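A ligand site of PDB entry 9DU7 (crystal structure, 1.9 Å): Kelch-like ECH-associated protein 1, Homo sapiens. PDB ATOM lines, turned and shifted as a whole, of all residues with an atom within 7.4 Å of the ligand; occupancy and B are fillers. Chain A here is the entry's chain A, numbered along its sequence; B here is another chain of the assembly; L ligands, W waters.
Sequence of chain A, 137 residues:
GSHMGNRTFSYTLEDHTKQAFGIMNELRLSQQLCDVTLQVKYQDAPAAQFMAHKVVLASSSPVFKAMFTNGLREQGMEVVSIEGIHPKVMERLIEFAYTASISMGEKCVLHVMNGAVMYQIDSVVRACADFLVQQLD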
ATOM      1  N   TYR A  42       5.106  26.968  13.756  1.00  0.00           N
ATOM      2  CA  TYR A  42       4.825  28.101  12.877  1.00  0.00           C
ATOM      3  C   TYR A  42       3.743  28.985  13.509  1.00  0.00           C
ATOM      4  O   TYR A  42       2.735  28.475  13.961  1.00  0.00           O
ATOM      5  CB  TYR A  42       4.329  27.616  11.513  1.00  0.00           C
ATOM      6  CG  TYR A  42       4.214  28.668  10.437  1.00  0.00           C
ATOM      7  CD1 TYR A  42       5.330  29.317   9.930  1.00  0.00           C
ATOM      8  CD2 TYR A  42       2.985  29.012   9.919  1.00  0.00           C
ATOM      9  CE1 TYR A  42       5.230  30.264   8.929  1.00  0.00           C
ATOM     10  CE2 TYR A  42       2.856  29.971   8.929  1.00  0.00           C
ATOM     11  CZ  TYR A  42       3.982  30.614   8.438  1.00  0.00           C
ATOM     12  OH  TYR A  42       3.840  31.533   7.454  1.00  0.00           O
ATOM     13  N   GLN A  43       3.986  30.296  13.506  1.00  0.00           N
ATOM     14  CA  GLN A  43       3.020  31.285  13.975  1.00  0.00           C
ATOM     15  C   GLN A  43       2.218  30.760  15.159  1.00  0.00           C
ATOM     16  O   GLN A  43       2.780  30.427  16.198  1.00  0.00           O
ATOM     17  CB  GLN A  43       2.107  31.688  12.820  1.00  0.00           C
ATOM     18  CG  GLN A  43       2.847  32.499  11.767  1.00  0.00           C
ATOM     19  CD  GLN A  43       1.995  32.781  10.548  1.00  0.00           C
ATOM     20  OE1 GLN A  43       2.498  33.258   9.534  1.00  0.00           O
ATOM     21  NE2 GLN A  43       0.721  32.458  10.631  1.00  0.00           N
ATOM     22  N   GLY A  84       9.178  28.799  11.470  1.00  0.00           N
ATOM     23  CA  GLY A  84       8.924  29.713  10.368  1.00  0.00           C
ATOM     24  C   GLY A  84       8.653  28.992   9.050  1.00  0.00           C
ATOM     25  O   GLY A  84       8.677  29.600   7.992  1.00  0.00           O
ATOM     26  N   ILE A  85       8.373  27.694   9.122  1.00  0.00           N
ATOM     27  CA  ILE A  85       7.822  26.976   7.994  1.00  0.00           C
ATOM     28  C   ILE A  85       6.588  26.251   8.473  1.00  0.00           C
ATOM     29  O   ILE A  85       6.624  25.521   9.466  1.00  0.00           O
ATOM     30  CB  ILE A  85       8.836  26.004   7.359  1.00  0.00           C
ATOM     31  CG1 ILE A  85       8.238  25.300   6.143  1.00  0.00           C
ATOM     32  CG2 ILE A  85       9.349  24.987   8.371  1.00  0.00           C
ATOM     33  CD1 ILE A  85       9.265  24.492   5.374  1.00  0.00           C
ATOM     34  N   HIS A  86       5.499  26.456   7.753  1.00  0.00           N
ATOM     35  CA  HIS A  86       4.241  25.830   8.072  1.00  0.00           C
ATOM     36  C   HIS A  86       4.363  24.317   7.976  1.00  0.00           C
ATOM     37  O   HIS A  86       4.949  23.798   7.025  1.00  0.00           O
ATOM     38  CB  HIS A  86       3.144  26.279   7.112  1.00  0.00           C
ATOM     39  CG  HIS A  86       1.776  26.055   7.656  1.00  0.00           C
ATOM     40  ND1 HIS A  86       1.173  24.809   7.637  1.00  0.00           N
ATOM     41  CD2 HIS A  86       0.876  26.910   8.191  1.00  0.00           C
ATOM     42  CE1 HIS A  86      -0.035  24.921   8.182  1.00  0.00           C
ATOM     43  NE2 HIS A  86      -0.242  26.184   8.502  1.00  0.00           N
ATOM     44  N   PRO A  87       3.815  23.591   8.971  1.00  0.00           N
ATOM     45  CA  PRO A  87       3.820  22.134   8.977  1.00  0.00           C
ATOM     46  C   PRO A  87       3.358  21.466   7.695  1.00  0.00           C
ATOM     47  O   PRO A  87       3.896  20.435   7.333  1.00  0.00           O
ATOM     48  CB  PRO A  87       2.816  21.800  10.096  1.00  0.00           C
ATOM     49  CG  PRO A  87       2.920  22.953  11.052  1.00  0.00           C
ATOM     50  CD  PRO A  87       3.238  24.154  10.202  1.00  0.00           C
ATOM     51  N   LYS A  88       2.354  22.035   7.026  1.00  0.00           N
ATOM     52  CA  LYS A  88       1.827  21.476   5.781  1.00  0.00           C
ATOM     53  C   LYS A  88       2.864  21.538   4.657  1.00  0.00           C
ATOM     54  O   LYS A  88       2.895  20.638   3.800  1.00  0.00           O
ATOM     55  CB  LYS A  88       0.547  22.210   5.378  1.00  0.00           C
ATOM     56  CG  LYS A  88      -0.663  21.782   6.204  1.00  0.00           C
ATOM     57  CD  LYS A  88      -1.934  22.583   5.962  1.00  0.00           C
ATOM     58  CE  LYS A  88      -3.044  22.168   6.904  1.00  0.00           C
ATOM     59  NZ  LYS A  88      -4.200  23.079   6.820  1.00  0.00           N
ATOM     60  N   VAL A  89       3.684  22.593   4.642  1.00  0.00           N
ATOM     61  CA  VAL A  89       4.775  22.698   3.678  1.00  0.00           C
ATOM     62  C   VAL A  89       5.786  21.595   3.960  1.00  0.00           C
ATOM     63  O   VAL A  89       6.137  20.823   3.079  1.00  0.00           O
ATOM     64  CB  VAL A  89       5.427  24.088   3.633  1.00  0.00           C
ATOM     65  CG1 VAL A  89       6.619  24.153   2.686  1.00  0.00           C
ATOM     66  CG2 VAL A  89       4.423  25.161   3.270  1.00  0.00           C
ATOM     67  N   MET A  90       6.230  21.515   5.220  1.00  0.00           N
ATOM     68  CA  MET A  90       7.227  20.539   5.589  1.00  0.00           C
ATOM     69  C   MET A  90       6.716  19.136   5.240  1.00  0.00           C
ATOM     70  O   MET A  90       7.513  18.293   4.842  1.00  0.00           O
ATOM     71  CB  MET A  90       7.541  20.594   7.080  1.00  0.00           C
ATOM     72  CG  MET A  90       8.560  19.547   7.533  1.00  0.00           C
ATOM     73  SD  MET A  90      10.154  19.785   6.714  1.00  0.00           S
ATOM     74  CE  MET A  90      10.382  21.561   6.922  1.00  0.00           C
ATOM     75  N   GLU A  91       5.452  18.864   5.566  1.00  0.00           N
ATOM     76  CA  GLU A  91       4.823  17.615   5.181  1.00  0.00           C
ATOM     77  C   GLU A  91       4.909  17.317   3.677  1.00  0.00           C
ATOM     78  O   GLU A  91       5.193  16.180   3.318  1.00  0.00           O
ATOM     79  CB  GLU A  91       3.350  17.594   5.560  1.00  0.00           C
ATOM     80  CG  GLU A  91       2.746  16.235   5.266  1.00  0.00           C
ATOM     81  CD  GLU A  91       1.439  16.000   5.993  1.00  0.00           C
ATOM     82  OE1 GLU A  91       0.503  16.730   5.687  1.00  0.00           O
ATOM     83  OE2 GLU A  91       1.392  15.128   6.870  1.00  0.00           O
ATOM     84  N   ARG A  92       4.650  18.294   2.809  1.00  0.00           N
ATOM     85  CA  ARG A  92       4.784  18.121   1.386  1.00  0.00           C
ATOM     86  C   ARG A  92       6.224  17.796   1.005  1.00  0.00           C
ATOM     87  O   ARG A  92       6.433  16.970   0.134  1.00  0.00           O
ATOM     88  CB  ARG A  92       4.355  19.345   0.580  1.00  0.00           C
ATOM     89  CG  ARG A  92       2.874  19.707   0.711  1.00  0.00           C
ATOM     90  CD  ARG A  92       1.901  18.721   0.144  1.00  0.00           C
ATOM     91  NE  ARG A  92       0.512  19.085   0.442  1.00  0.00           N
ATOM     92  CZ  ARG A  92      -0.266  19.893  -0.258  1.00  0.00           C
ATOM     93  NH1 ARG A  92       0.140  20.406  -1.395  1.00  0.00           N
ATOM     94  NH2 ARG A  92      -1.477  20.211   0.182  1.00  0.00           N
ATOM     95  N   SER A 103       2.930  17.628  -4.513  1.00  0.00           N
ATOM     96  CA  SER A 103       1.559  18.094  -4.682  1.00  0.00           C
ATOM     97  C   SER A 103       1.457  19.580  -4.380  1.00  0.00           C
ATOM     98  O   SER A 103       2.066  20.048  -3.419  1.00  0.00           O
ATOM     99  CB  SER A 103       0.654  17.357  -3.768  1.00  0.00           C
ATOM    100  OG  SER A 103       0.705  15.991  -4.062  1.00  0.00           O
ATOM    101  N   MET A 104       0.607  20.268  -5.156  1.00  0.00           N
ATOM    102  CA  MET A 104       0.391  21.697  -4.993  1.00  0.00           C
ATOM    103  C   MET A 104      -0.942  22.069  -5.633  1.00  0.00           C
ATOM    104  O   MET A 104      -1.477  21.328  -6.462  1.00  0.00           O
ATOM    105  CB  MET A 104       1.488  22.545  -5.661  1.00  0.00           C
ATOM    106  CG  MET A 104       1.620  22.265  -7.137  1.00  0.00           C
ATOM    107  SD  MET A 104       3.118  22.901  -7.959  1.00  0.00           S
ATOM    108  CE  MET A 104       4.279  21.636  -7.424  1.00  0.00           C
ATOM    109  N   GLY A 105      -1.376  23.295  -5.314  1.00  0.00           N
ATOM    110  CA  GLY A 105      -2.493  23.941  -5.977  1.00  0.00           C
ATOM    111  C   GLY A 105      -2.318  25.454  -5.929  1.00  0.00           C
ATOM    112  O   GLY A 105      -1.393  25.972  -5.302  1.00  0.00           O
ATOM    113  N   GLU A 106      -3.284  26.138  -6.565  1.00  0.00           N
ATOM    114  CA  GLU A 106      -3.276  27.584  -6.762  1.00  0.00           C
ATOM    115  C   GLU A 106      -2.917  28.297  -5.468  1.00  0.00           C
ATOM    116  O   GLU A 106      -2.059  29.168  -5.481  1.00  0.00           O
ATOM    117  CB  GLU A 106      -4.651  28.017  -7.299  1.00  0.00           C
ATOM    118  CG  GLU A 106      -4.835  29.501  -7.580  1.00  0.00           C
ATOM    119  CD  GLU A 106      -6.293  29.942  -7.777  1.00  0.00           C
ATOM    120  OE1 GLU A 106      -7.218  29.103  -7.642  1.00  0.00           O
ATOM    121  OE2 GLU A 106      -6.513  31.150  -8.043  1.00  0.00           O
ATOM    122  N   LYS A 107      -3.542  27.892  -4.355  1.00  0.00           N
ATOM    123  CA  LYS A 107      -3.426  28.672  -3.137  1.00  0.00           C
ATOM    124  C   LYS A 107      -2.236  28.252  -2.279  1.00  0.00           C
ATOM    125  O   LYS A 107      -1.994  28.868  -1.238  1.00  0.00           O
ATOM    126  CB  LYS A 107      -4.698  28.541  -2.290  1.00  0.00           C
ATOM    127  CG  LYS A 107      -5.895  29.305  -2.838  1.00  0.00           C
ATOM    128  CD  LYS A 107      -7.218  28.706  -2.426  1.00  0.00           C
ATOM    129  CE  LYS A 107      -8.368  29.676  -2.604  1.00  0.00           C
ATOM    130  NZ  LYS A 107      -9.642  29.134  -2.049  1.00  0.00           N
ATOM    131  N   CYS A 108      -1.491  27.195  -2.651  1.00  0.00           N
ATOM    132  CA  CYS A 108      -0.350  26.821  -1.830  1.00  0.00           C
ATOM    133  C   CYS A 108       0.960  26.697  -2.628  1.00  0.00           C
ATOM    134  O   CYS A 108       1.955  26.387  -2.002  1.00  0.00           O
ATOM    135  CB  CYS A 108      -0.537  25.505  -1.065  1.00  0.00           C
ATOM    136  SG  CYS A 108      -0.983  24.028  -1.959  1.00  0.00           S
ATOM    137  N   VAL A 109       0.943  26.959  -3.925  1.00  0.00           N
ATOM    138  CA  VAL A 109       2.139  26.744  -4.734  1.00  0.00           C
ATOM    139  C   VAL A 109       3.251  27.661  -4.237  1.00  0.00           C
ATOM    140  O   VAL A 109       4.389  27.228  -4.152  1.00  0.00           O
ATOM    141  CB  VAL A 109       1.927  26.861  -6.250  1.00  0.00           C
ATOM    142  CG1 VAL A 109       1.291  28.185  -6.684  1.00  0.00           C
ATOM    143  CG2 VAL A 109       3.241  26.626  -6.994  1.00  0.00           C
ATOM    144  N   HIS A 111       3.687  28.752  -1.224  1.00  0.00           N
ATOM    145  CA  HIS A 111       4.132  28.233   0.034  1.00  0.00           C
ATOM    146  C   HIS A 111       5.066  27.037  -0.165  1.00  0.00           C
ATOM    147  O   HIS A 111       6.068  26.911   0.532  1.00  0.00           O
ATOM    148  CB  HIS A 111       2.946  27.844   0.898  1.00  0.00           C
ATOM    149  CG  HIS A 111       2.099  28.999   1.315  1.00  0.00           C
ATOM    150  ND1 HIS A 111       0.718  28.935   1.346  1.00  0.00           N
ATOM    151  CD2 HIS A 111       2.424  30.215   1.753  1.00  0.00           C
ATOM    152  CE1 HIS A 111       0.244  30.100   1.744  1.00  0.00           C
ATOM    153  NE2 HIS A 111       1.261  30.891   1.986  1.00  0.00           N
ATOM    154  N   VAL A 112       4.693  26.119  -1.061  1.00  0.00           N
ATOM    155  CA  VAL A 112       5.529  24.963  -1.357  1.00  0.00           C
ATOM    156  C   VAL A 112       6.842  25.427  -1.970  1.00  0.00           C
ATOM    157  O   VAL A 112       7.909  24.921  -1.611  1.00  0.00           O
ATOM    158  CB  VAL A 112       4.829  23.954  -2.284  1.00  0.00           C
ATOM    159  CG1 VAL A 112       5.759  22.790  -2.647  1.00  0.00           C
ATOM    160  CG2 VAL A 112       3.573  23.427  -1.608  1.00  0.00           C
ATOM    161  N   ASN A 114       8.377  28.237  -1.529  1.00  0.00           N
ATOM    162  CA  ASN A 114       9.193  28.862  -0.478  1.00  0.00           C
ATOM    163  C   ASN A 114       9.966  27.799   0.313  1.00  0.00           C
ATOM    164  O   ASN A 114      11.177  27.922   0.561  1.00  0.00           O
ATOM    165  CB  ASN A 114       8.308  29.726   0.407  1.00  0.00           C
ATOM    166  CG  ASN A 114       9.110  30.439   1.464  1.00  0.00           C
ATOM    167  OD1 ASN A 114      10.118  31.047   1.155  1.00  0.00           O
ATOM    168  ND2 ASN A 114       8.768  30.265   2.721  1.00  0.00           N
ATOM    169  N   ASN B   6      -9.772  24.672  -5.640  1.00  0.00           N
ATOM    170  CA  ASN B   6      -9.043  23.976  -4.594  1.00  0.00           C
ATOM    171  C   ASN B   6      -8.562  22.612  -5.090  1.00  0.00           C
ATOM    172  O   ASN B   6      -8.372  21.681  -4.296  1.00  0.00           O
ATOM    173  CB  ASN B   6      -9.900  23.906  -3.328  1.00  0.00           C
ATOM    174  CG  ASN B   6      -9.766  25.140  -2.448  1.00  0.00           C
ATOM    175  OD1 ASN B   6      -9.453  26.214  -2.926  1.00  0.00           O
ATOM    176  ND2 ASN B   6      -9.924  24.980  -1.144  1.00  0.00           N
ATOM    177  N   ARG B   7      -8.389  22.475  -6.409  1.00  0.00           N
ATOM    178  CA  ARG B   7      -7.900  21.222  -6.980  1.00  0.00           C
ATOM    179  C   ARG B   7      -6.404  21.089  -6.660  1.00  0.00           C
ATOM    180  O   ARG B   7      -5.709  22.096  -6.621  1.00  0.00           O
ATOM    181  CB  ARG B   7      -8.068  21.177  -8.490  1.00  0.00           C
ATOM    182  CG  ARG B   7      -7.591  19.878  -9.096  1.00  0.00           C
ATOM    183  CD  ARG B   7      -7.914  19.769 -10.565  1.00  0.00           C
ATOM    184  NE  ARG B   7      -7.579  18.437 -11.013  1.00  0.00           N
ATOM    185  CZ  ARG B   7      -7.848  17.972 -12.229  1.00  0.00           C
ATOM    186  NH1 ARG B   7      -8.428  18.764 -13.121  1.00  0.00           N
ATOM    187  NH2 ARG B   7      -7.554  16.718 -12.541  1.00  0.00           N
ATOM    188  N   THR B   8      -5.952  19.863  -6.404  1.00  0.00           N
ATOM    189  CA  THR B   8      -4.534  19.617  -6.140  1.00  0.00           C
ATOM    190  C   THR B   8      -4.000  18.744  -7.251  1.00  0.00           C
ATOM    191  O   THR B   8      -4.668  17.810  -7.723  1.00  0.00           O
ATOM    192  CB  THR B   8      -4.247  19.039  -4.733  1.00  0.00           C
ATOM    193  OG1 THR B   8      -5.133  17.962  -4.416  1.00  0.00           O
ATOM    194  CG2 THR B   8      -4.333  20.090  -3.652  1.00  0.00           C
HETATM  195  C1  LIG L   1      -3.754  23.363  -0.120  1.00  0.00           C
HETATM  196  C2  LIG L   1      -3.879  21.914   1.837  1.00  0.00           C
HETATM  197  C3  LIG L   1      -4.841  21.848   2.985  1.00  0.00           C
HETATM  198  C4  LIG L   1      -4.630  24.165   3.385  1.00  0.00           C
HETATM  199  C5  LIG L   1      -3.799  24.412   2.132  1.00  0.00           C
HETATM  200  C6  LIG L   1      -2.350  24.725   2.436  1.00  0.00           C
HETATM  201  C7  LIG L   1      -1.285  23.946   1.908  1.00  0.00           C
HETATM  202  C8  LIG L   1      -0.345  27.305   4.312  1.00  0.00           C
HETATM  203  C9  LIG L   1       1.296  28.657   5.250  1.00  0.00           C
HETATM  204  C10 LIG L   1      -0.951  29.162   5.627  1.00  0.00           C
HETATM  205 CL1  LIG L   1       1.411  23.277   1.543  1.00  0.00          CL
HETATM  206  C11 LIG L   1       0.057  24.287   2.168  1.00  0.00           C
HETATM  207  O1  LIG L   1      -4.436  22.844   3.891  1.00  0.00           O
HETATM  208  N1  LIG L   1      -3.853  23.263   1.219  1.00  0.00           N
HETATM  209  O2  LIG L   1      -3.714  22.325  -0.797  1.00  0.00           O
HETATM  210  C12 LIG L   1      -3.519  24.644  -0.856  1.00  0.00           C
HETATM  211  C13 LIG L   1      -2.766  24.290  -2.173  1.00  0.00           C
HETATM  212  C14 LIG L   1       0.334  25.395   2.951  1.00  0.00           C
HETATM  213  C15 LIG L   1      -0.708  26.155   3.469  1.00  0.00           C
HETATM  214  C16 LIG L   1      -2.038  25.843   3.211  1.00  0.00           C
HETATM  215  N2  LIG L   1      -1.295  28.097   4.856  1.00  0.00           N
HETATM  216  N3  LIG L   1       0.346  29.454   5.822  1.00  0.00           N
HETATM  217  N4  LIG L   1       0.962  27.586   4.495  1.00  0.00           N
HETATM  218  N5  LIG L   1       2.596  28.924   5.471  1.00  0.00           N
HETATM  219  O   HOH W   1       5.355  28.112   5.374  1.00  0.00           O
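SG of Cys 108 is covalently linked to C13 of the ligand, at 1.8 Å.
The side-chain amino group of Lys 88 sits at hydrogen-bond distance from an oxygen (O1) of the ligand (2.9 Å).
An oxygen (O2) of the ligand lies within hydrogen-bond range of the guanidinium group of Arg 92 (3.2 Å).
ND1 of His 111 is in hydrogen-bond range of N4 of the ligand (3.4 Å).
N of Gly 105 sits at hydrogen-bond distance from SG of Cys 108 (3.5 Å).
The backbone NH of Lys 88 sits at hydrogen-bond distance from a ring nitrogen (ND1) of His 86 (3.1 Å).
O of Ser 103 lies within hydrogen-bond range of NH1 of Arg 92, 2.8 Å away.
OE1 of Gln 43 lies within hydrogen-bond range of OH of Tyr 42.
NZ of Lys 107 is in hydrogen-bond range of OD1 of Asn 6 of chain B (3.1 Å).
Merely in contact with the ligand: Tyr 42 (3.5 Å), His 86 (3.2 Å), Val 89 (3.9 Å), Gly 105 (3.6 Å), Lys 107 (3.999 Å), Val 112 (3.8 Å) and Thr 8 of chain B (3.7 Å).
Hydrophobic or aromatic side chains within 4 Å of the ligand: Tyr 42, His 86, Val 89, His 111 and Val 112.
Of the 24 residues printed, 11 come within 4 Å of the ligand.
The nearest printed residue that does not touch the ligand is Met 104 (4.5 Å).
Water W1 bridges a nitrogen (N5) of the ligand and the backbone NH (N) of His 86.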
